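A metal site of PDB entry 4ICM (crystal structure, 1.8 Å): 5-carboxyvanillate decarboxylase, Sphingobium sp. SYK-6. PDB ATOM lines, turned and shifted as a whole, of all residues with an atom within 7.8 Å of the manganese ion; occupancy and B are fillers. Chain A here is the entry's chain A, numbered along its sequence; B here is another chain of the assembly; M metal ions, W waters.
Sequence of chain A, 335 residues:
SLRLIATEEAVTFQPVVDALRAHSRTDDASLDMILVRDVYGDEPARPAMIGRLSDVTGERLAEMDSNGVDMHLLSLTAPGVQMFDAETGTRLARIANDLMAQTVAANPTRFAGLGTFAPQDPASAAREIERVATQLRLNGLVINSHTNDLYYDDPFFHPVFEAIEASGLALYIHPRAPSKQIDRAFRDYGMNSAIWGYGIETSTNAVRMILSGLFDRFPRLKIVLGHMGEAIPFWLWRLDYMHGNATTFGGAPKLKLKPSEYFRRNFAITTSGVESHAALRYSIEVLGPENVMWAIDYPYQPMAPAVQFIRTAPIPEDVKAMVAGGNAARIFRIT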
ATOM      1  N   GLU A   8     -21.697 -36.355  13.848  1.00  0.00           N
ATOM      2  CA  GLU A   8     -21.667 -35.179  12.969  1.00  0.00           C
ATOM      3  C   GLU A   8     -20.270 -34.599  12.940  1.00  0.00           C
ATOM      4  O   GLU A   8     -20.047 -33.444  13.325  1.00  0.00           O
ATOM      5  CB  GLU A   8     -22.683 -34.116  13.398  1.00  0.00           C
ATOM      6  CG  GLU A   8     -23.010 -33.111  12.282  1.00  0.00           C
ATOM      7  CD  GLU A   8     -23.865 -31.951  12.750  1.00  0.00           C
ATOM      8  OE1 GLU A   8     -25.036 -32.184  13.147  1.00  0.00           O
ATOM      9  OE2 GLU A   8     -23.394 -30.804  12.718  1.00  0.00           O
ATOM     10  N   GLU A   9     -19.320 -35.405  12.499  1.00  0.00           N
ATOM     11  CA  GLU A   9     -17.925 -35.038  12.636  1.00  0.00           C
ATOM     12  C   GLU A   9     -17.348 -34.667  11.284  1.00  0.00           C
ATOM     13  O   GLU A   9     -17.225 -35.505  10.401  1.00  0.00           O
ATOM     14  CB  GLU A   9     -17.154 -36.180  13.296  1.00  0.00           C
ATOM     15  CG  GLU A   9     -17.927 -36.746  14.491  1.00  0.00           C
ATOM     16  CD  GLU A   9     -18.450 -35.631  15.415  1.00  0.00           C
ATOM     17  OE1 GLU A   9     -19.641 -35.674  15.808  1.00  0.00           O
ATOM     18  OE2 GLU A   9     -17.663 -34.726  15.746  1.00  0.00           O
ATOM     19  N   ALA A  10     -17.020 -33.394  11.132  1.00  0.00           N
ATOM     20  CA  ALA A  10     -16.625 -32.836   9.848  1.00  0.00           C
ATOM     21  C   ALA A  10     -15.194 -33.207   9.433  1.00  0.00           C
ATOM     22  O   ALA A  10     -14.312 -33.357  10.278  1.00  0.00           O
ATOM     23  CB  ALA A  10     -16.801 -31.336   9.862  1.00  0.00           C
ATOM     24  N   SER A  75     -18.109 -36.709   7.829  1.00  0.00           N
ATOM     25  CA  SER A  75     -18.861 -36.136   6.719  1.00  0.00           C
ATOM     26  C   SER A  75     -18.073 -34.984   6.108  1.00  0.00           C
ATOM     27  O   SER A  75     -17.470 -34.190   6.833  1.00  0.00           O
ATOM     28  CB  SER A  75     -20.238 -35.648   7.203  1.00  0.00           C
ATOM     29  OG  SER A  75     -20.132 -34.882   8.392  1.00  0.00           O
ATOM     30  N   THR A  77     -17.295 -31.573   5.193  1.00  0.00           N
ATOM     31  CA  THR A  77     -17.779 -30.382   5.871  1.00  0.00           C
ATOM     32  C   THR A  77     -18.633 -29.510   4.929  1.00  0.00           C
ATOM     33  O   THR A  77     -18.434 -29.507   3.709  1.00  0.00           O
ATOM     34  CB  THR A  77     -16.576 -29.577   6.417  1.00  0.00           C
ATOM     35  OG1 THR A  77     -17.035 -28.540   7.294  1.00  0.00           O
ATOM     36  CG2 THR A  77     -15.771 -28.971   5.284  1.00  0.00           C
ATOM     37  N   ALA A  78     -19.583 -28.782   5.510  1.00  0.00           N
ATOM     38  CA  ALA A  78     -20.345 -27.794   4.767  1.00  0.00           C
ATOM     39  C   ALA A  78     -19.406 -26.724   4.248  1.00  0.00           C
ATOM     40  O   ALA A  78     -18.440 -26.357   4.937  1.00  0.00           O
ATOM     41  CB  ALA A  78     -21.428 -27.159   5.655  1.00  0.00           C
ATOM     42  N   ASN A 144     -25.789 -30.590   2.648  1.00  0.00           N
ATOM     43  CA  ASN A 144     -25.876 -29.384   3.474  1.00  0.00           C
ATOM     44  C   ASN A 144     -27.009 -28.452   3.064  1.00  0.00           C
ATOM     45  O   ASN A 144     -26.840 -27.606   2.204  1.00  0.00           O
ATOM     46  CB  ASN A 144     -24.545 -28.646   3.410  1.00  0.00           C
ATOM     47  CG  ASN A 144     -23.392 -29.552   3.717  1.00  0.00           C
ATOM     48  OD1 ASN A 144     -23.187 -29.918   4.863  1.00  0.00           O
ATOM     49  ND2 ASN A 144     -22.651 -29.973   2.672  1.00  0.00           N
ATOM     50  N   TYR A 172     -28.230 -37.464   6.274  1.00  0.00           N
ATOM     51  CA  TYR A 172     -28.007 -36.413   7.251  1.00  0.00           C
ATOM     52  C   TYR A 172     -28.083 -35.082   6.521  1.00  0.00           C
ATOM     53  O   TYR A 172     -27.274 -34.804   5.648  1.00  0.00           O
ATOM     54  CB  TYR A 172     -26.603 -36.574   7.869  1.00  0.00           C
ATOM     55  CG  TYR A 172     -26.423 -35.983   9.254  1.00  0.00           C
ATOM     56  CD1 TYR A 172     -26.748 -34.659   9.520  1.00  0.00           C
ATOM     57  CD2 TYR A 172     -25.940 -36.754  10.307  1.00  0.00           C
ATOM     58  CE1 TYR A 172     -26.574 -34.117  10.784  1.00  0.00           C
ATOM     59  CE2 TYR A 172     -25.771 -36.233  11.569  1.00  0.00           C
ATOM     60  CZ  TYR A 172     -26.093 -34.911  11.810  1.00  0.00           C
ATOM     61  OH  TYR A 172     -25.921 -34.377  13.063  1.00  0.00           O
ATOM     62  N   HIS A 174     -27.285 -31.657   6.978  1.00  0.00           N
ATOM     63  CA  HIS A 174     -26.447 -30.806   7.812  1.00  0.00           C
ATOM     64  C   HIS A 174     -26.749 -29.360   7.445  1.00  0.00           C
ATOM     65  O   HIS A 174     -27.268 -29.090   6.362  1.00  0.00           O
ATOM     66  CB  HIS A 174     -24.986 -31.166   7.486  1.00  0.00           C
ATOM     67  CG  HIS A 174     -23.977 -30.469   8.342  1.00  0.00           C
ATOM     68  ND1 HIS A 174     -23.583 -29.170   8.121  1.00  0.00           N
ATOM     69  CD2 HIS A 174     -23.236 -30.915   9.386  1.00  0.00           C
ATOM     70  CE1 HIS A 174     -22.679 -28.826   9.012  1.00  0.00           C
ATOM     71  NE2 HIS A 174     -22.433 -29.878   9.784  1.00  0.00           N
ATOM     72  N   PRO A 175     -26.461 -28.413   8.357  1.00  0.00           N
ATOM     73  CA  PRO A 175     -26.733 -27.034   7.951  1.00  0.00           C
ATOM     74  C   PRO A 175     -25.802 -26.474   6.874  1.00  0.00           C
ATOM     75  O   PRO A 175     -24.739 -27.022   6.574  1.00  0.00           O
ATOM     76  CB  PRO A 175     -26.535 -26.228   9.242  1.00  0.00           C
ATOM     77  CG  PRO A 175     -26.840 -27.202  10.313  1.00  0.00           C
ATOM     78  CD  PRO A 175     -26.262 -28.506   9.814  1.00  0.00           C
ATOM     79  N   TYR A 198     -28.017 -21.104  10.628  1.00  0.00           N
ATOM     80  CA  TYR A 198     -27.941 -22.540  10.314  1.00  0.00           C
ATOM     81  C   TYR A 198     -29.261 -23.268  10.655  1.00  0.00           C
ATOM     82  O   TYR A 198     -29.802 -23.995   9.828  1.00  0.00           O
ATOM     83  CB  TYR A 198     -26.758 -23.190  11.046  1.00  0.00           C
ATOM     84  CG  TYR A 198     -25.423 -23.003  10.330  1.00  0.00           C
ATOM     85  CD1 TYR A 198     -25.310 -22.165   9.225  1.00  0.00           C
ATOM     86  CD2 TYR A 198     -24.282 -23.679  10.749  1.00  0.00           C
ATOM     87  CE1 TYR A 198     -24.086 -21.995   8.555  1.00  0.00           C
ATOM     88  CE2 TYR A 198     -23.043 -23.517  10.082  1.00  0.00           C
ATOM     89  CZ  TYR A 198     -22.964 -22.684   9.002  1.00  0.00           C
ATOM     90  OH  TYR A 198     -21.771 -22.520   8.334  1.00  0.00           O
ATOM     91  N   GLY A 226     -29.159 -32.640  12.875  1.00  0.00           N
ATOM     92  CA  GLY A 226     -28.330 -32.351  14.023  1.00  0.00           C
ATOM     93  C   GLY A 226     -28.912 -31.222  14.864  1.00  0.00           C
ATOM     94  O   GLY A 226     -30.043 -30.782  14.622  1.00  0.00           O
ATOM     95  N   HIS A 227     -28.146 -30.764  15.843  1.00  0.00           N
ATOM     96  CA  HIS A 227     -28.530 -29.610  16.668  1.00  0.00           C
ATOM     97  C   HIS A 227     -29.900 -29.772  17.282  1.00  0.00           C
ATOM     98  O   HIS A 227     -30.756 -28.889  17.207  1.00  0.00           O
ATOM     99  CB  HIS A 227     -28.375 -28.323  15.858  1.00  0.00           C
ATOM    100  CG  HIS A 227     -27.131 -28.332  15.027  1.00  0.00           C
ATOM    101  ND1 HIS A 227     -27.148 -28.462  13.650  1.00  0.00           N
ATOM    102  CD2 HIS A 227     -25.824 -28.347  15.397  1.00  0.00           C
ATOM    103  CE1 HIS A 227     -25.905 -28.499  13.205  1.00  0.00           C
ATOM    104  NE2 HIS A 227     -25.075 -28.442  14.243  1.00  0.00           N
ATOM    105  N   GLU A 230     -32.766 -29.388  14.876  1.00  0.00           N
ATOM    106  CA  GLU A 230     -32.957 -27.999  14.457  1.00  0.00           C
ATOM    107  C   GLU A 230     -34.240 -27.390  15.027  1.00  0.00           C
ATOM    108  O   GLU A 230     -34.965 -26.649  14.345  1.00  0.00           O
ATOM    109  CB  GLU A 230     -32.844 -27.874  12.934  1.00  0.00           C
ATOM    110  CG  GLU A 230     -31.622 -28.619  12.350  1.00  0.00           C
ATOM    111  CD  GLU A 230     -30.263 -27.936  12.608  1.00  0.00           C
ATOM    112  OE1 GLU A 230     -30.222 -26.857  13.247  1.00  0.00           O
ATOM    113  OE2 GLU A 230     -29.220 -28.477  12.173  1.00  0.00           O
ATOM    114  N   SER A 272     -25.672 -32.646  18.391  1.00  0.00           N
ATOM    115  CA  SER A 272     -24.542 -31.794  18.040  1.00  0.00           C
ATOM    116  C   SER A 272     -24.793 -30.345  18.435  1.00  0.00           C
ATOM    117  O   SER A 272     -25.819 -29.780  18.106  1.00  0.00           O
ATOM    118  CB  SER A 272     -24.258 -31.855  16.543  1.00  0.00           C
ATOM    119  OG  SER A 272     -25.420 -31.551  15.803  1.00  0.00           O
ATOM    120  N   GLY A 273     -23.853 -29.743  19.144  1.00  0.00           N
ATOM    121  CA  GLY A 273     -23.984 -28.348  19.483  1.00  0.00           C
ATOM    122  C   GLY A 273     -25.110 -27.988  20.431  1.00  0.00           C
ATOM    123  O   GLY A 273     -25.424 -26.813  20.568  1.00  0.00           O
ATOM    124  N   ILE A 296     -20.680 -34.760  18.363  1.00  0.00           N
ATOM    125  CA  ILE A 296     -19.780 -33.758  18.900  1.00  0.00           C
ATOM    126  C   ILE A 296     -19.836 -32.457  18.110  1.00  0.00           C
ATOM    127  O   ILE A 296     -19.900 -31.377  18.707  1.00  0.00           O
ATOM    128  CB  ILE A 296     -18.331 -34.257  18.896  1.00  0.00           C
ATOM    129  CG1 ILE A 296     -18.183 -35.510  19.767  1.00  0.00           C
ATOM    130  CG2 ILE A 296     -17.378 -33.164  19.385  1.00  0.00           C
ATOM    131  CD1 ILE A 296     -16.795 -36.182  19.629  1.00  0.00           C
ATOM    132  N   ASP A 297     -19.803 -32.582  16.779  1.00  0.00           N
ATOM    133  CA  ASP A 297     -19.642 -31.466  15.839  1.00  0.00           C
ATOM    134  C   ASP A 297     -18.200 -30.951  15.842  1.00  0.00           C
ATOM    135  O   ASP A 297     -17.954 -29.751  15.767  1.00  0.00           O
ATOM    136  CB  ASP A 297     -20.625 -30.312  16.139  1.00  0.00           C
ATOM    137  CG  ASP A 297     -21.169 -29.650  14.887  1.00  0.00           C
ATOM    138  OD1 ASP A 297     -20.676 -29.973  13.775  1.00  0.00           O
ATOM    139  OD2 ASP A 297     -22.088 -28.815  15.019  1.00  0.00           O
ATOM    140  N   TYR A 298     -17.266 -31.885  15.961  1.00  0.00           N
ATOM    141  CA  TYR A 298     -15.851 -31.602  15.869  1.00  0.00           C
ATOM    142  C   TYR A 298     -15.578 -31.257  14.401  1.00  0.00           C
ATOM    143  O   TYR A 298     -16.203 -31.832  13.512  1.00  0.00           O
ATOM    144  CB  TYR A 298     -15.059 -32.853  16.282  1.00  0.00           C
ATOM    145  CG  TYR A 298     -13.558 -32.691  16.224  1.00  0.00           C
ATOM    146  CD1 TYR A 298     -12.865 -32.125  17.283  1.00  0.00           C
ATOM    147  CD2 TYR A 298     -12.840 -33.093  15.105  1.00  0.00           C
ATOM    148  CE1 TYR A 298     -11.478 -31.971  17.241  1.00  0.00           C
ATOM    149  CE2 TYR A 298     -11.446 -32.943  15.048  1.00  0.00           C
ATOM    150  CZ  TYR A 298     -10.780 -32.386  16.117  1.00  0.00           C
ATOM    151  OH  TYR A 298      -9.413 -32.228  16.085  1.00  0.00           O
ATOM    152  N   PRO A 299     -14.653 -30.327  14.138  1.00  0.00           N
ATOM    153  CA  PRO A 299     -13.793 -29.575  15.062  1.00  0.00           C
ATOM    154  C   PRO A 299     -14.351 -28.228  15.472  1.00  0.00           C
ATOM    155  O   PRO A 299     -13.656 -27.440  16.109  1.00  0.00           O
ATOM    156  CB  PRO A 299     -12.521 -29.371  14.221  1.00  0.00           C
ATOM    157  CG  PRO A 299     -13.050 -29.211  12.839  1.00  0.00           C
ATOM    158  CD  PRO A 299     -14.230 -30.163  12.731  1.00  0.00           C
ATOM    159  N   TYR A 300     -15.600 -27.959  15.121  1.00  0.00           N
ATOM    160  CA  TYR A 300     -16.238 -26.692  15.459  1.00  0.00           C
ATOM    161  C   TYR A 300     -16.582 -26.670  16.941  1.00  0.00           C
ATOM    162  O   TYR A 300     -16.738 -25.603  17.520  1.00  0.00           O
ATOM    163  CB  TYR A 300     -17.475 -26.479  14.587  1.00  0.00           C
ATOM    164  CG  TYR A 300     -17.134 -26.515  13.115  1.00  0.00           C
ATOM    165  CD1 TYR A 300     -16.576 -25.411  12.474  1.00  0.00           C
ATOM    166  CD2 TYR A 300     -17.360 -27.671  12.362  1.00  0.00           C
ATOM    167  CE1 TYR A 300     -16.256 -25.448  11.123  1.00  0.00           C
ATOM    168  CE2 TYR A 300     -17.038 -27.716  11.009  1.00  0.00           C
ATOM    169  CZ  TYR A 300     -16.485 -26.601  10.395  1.00  0.00           C
ATOM    170  OH  TYR A 300     -16.168 -26.652   9.054  1.00  0.00           O
ATOM    171  N   GLN A 301     -16.698 -27.847  17.533  1.00  0.00           N
ATOM    172  CA  GLN A 301     -16.889 -27.995  18.975  1.00  0.00           C
ATOM    173  C   GLN A 301     -15.817 -28.938  19.511  1.00  0.00           C
ATOM    174  O   GLN A 301     -15.417 -29.871  18.807  1.00  0.00           O
ATOM    175  CB  GLN A 301     -18.261 -28.597  19.289  1.00  0.00           C
ATOM    176  CG  GLN A 301     -19.446 -27.878  18.642  1.00  0.00           C
ATOM    177  CD  GLN A 301     -20.292 -27.162  19.666  1.00  0.00           C
ATOM    178  OE1 GLN A 301     -20.076 -27.289  20.872  1.00  0.00           O
ATOM    179  NE2 GLN A 301     -21.280 -26.412  19.183  1.00  0.00           N
ATOM    180  N   ARG B 238     -27.181 -23.255  22.554  1.00  0.00           N
ATOM    181  CA  ARG B 238     -26.481 -22.983  21.292  1.00  0.00           C
ATOM    182  C   ARG B 238     -26.326 -21.477  21.035  1.00  0.00           C
ATOM    183  O   ARG B 238     -25.291 -21.039  20.544  1.00  0.00           O
ATOM    184  CB  ARG B 238     -27.242 -23.652  20.140  1.00  0.00           C
ATOM    185  CG  ARG B 238     -26.578 -23.535  18.770  1.00  0.00           C
ATOM    186  CD  ARG B 238     -26.852 -24.810  18.024  1.00  0.00           C
ATOM    187  NE  ARG B 238     -26.579 -24.765  16.590  1.00  0.00           N
ATOM    188  CZ  ARG B 238     -25.435 -25.107  16.031  1.00  0.00           C
ATOM    189  NH1 ARG B 238     -24.392 -25.473  16.788  1.00  0.00           N
ATOM    190  NH2 ARG B 238     -25.310 -25.064  14.707  1.00  0.00           N
HETATM  191 MN    MN M   1     -21.694 -29.714  11.862  1.00  0.00          MN
HETATM  192  O   HOH W   1     -22.718 -27.697  12.184  1.00  0.00           O
HETATM  193  O   HOH W   2     -20.277 -31.490  11.248  1.00  0.00           O
HETATM  194  O   HOH W   3     -20.127 -28.331  11.176  1.00  0.00           O
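NE2 of His 227 lies within hydrogen-bond range of OD2 of Asp 297, at 3.1 Å. The side-chain carboxylate (OE1) of Glu 8 sits at hydrogen-bond distance from the side-chain hydroxyl (OG) of Ser 272 (2.8 Å). The backbone NH (N) of Asp 297 lies within hydrogen-bond range of the side-chain carboxylate (OE2) of Glu 9 (3.2 Å). A ring nitrogen (ND1) of His 174 is in hydrogen-bond range of the side-chain amide oxygen (OD1) of Asn 144 (3.4 Å). OE2 of Glu 8 lies close to NE2 of His 227 (3.3 Å).
Water W1 bridges OD2 of Asp 297 (3.1 Å) and NE2 of His 227 (3.2 Å).
The manganese ion is bound by OD1 of Asp 297 (2.2 Å). OE2 of Glu 8 binds the manganese ion. Water W3 is bound to the manganese ion. The manganese ion is bound by a ring nitrogen (NE2) of His 174 (2.2 Å). The manganese ion is bound by water W1, 2.3 Å away. The manganese ion is bound by water W2, at 2.4 Å.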
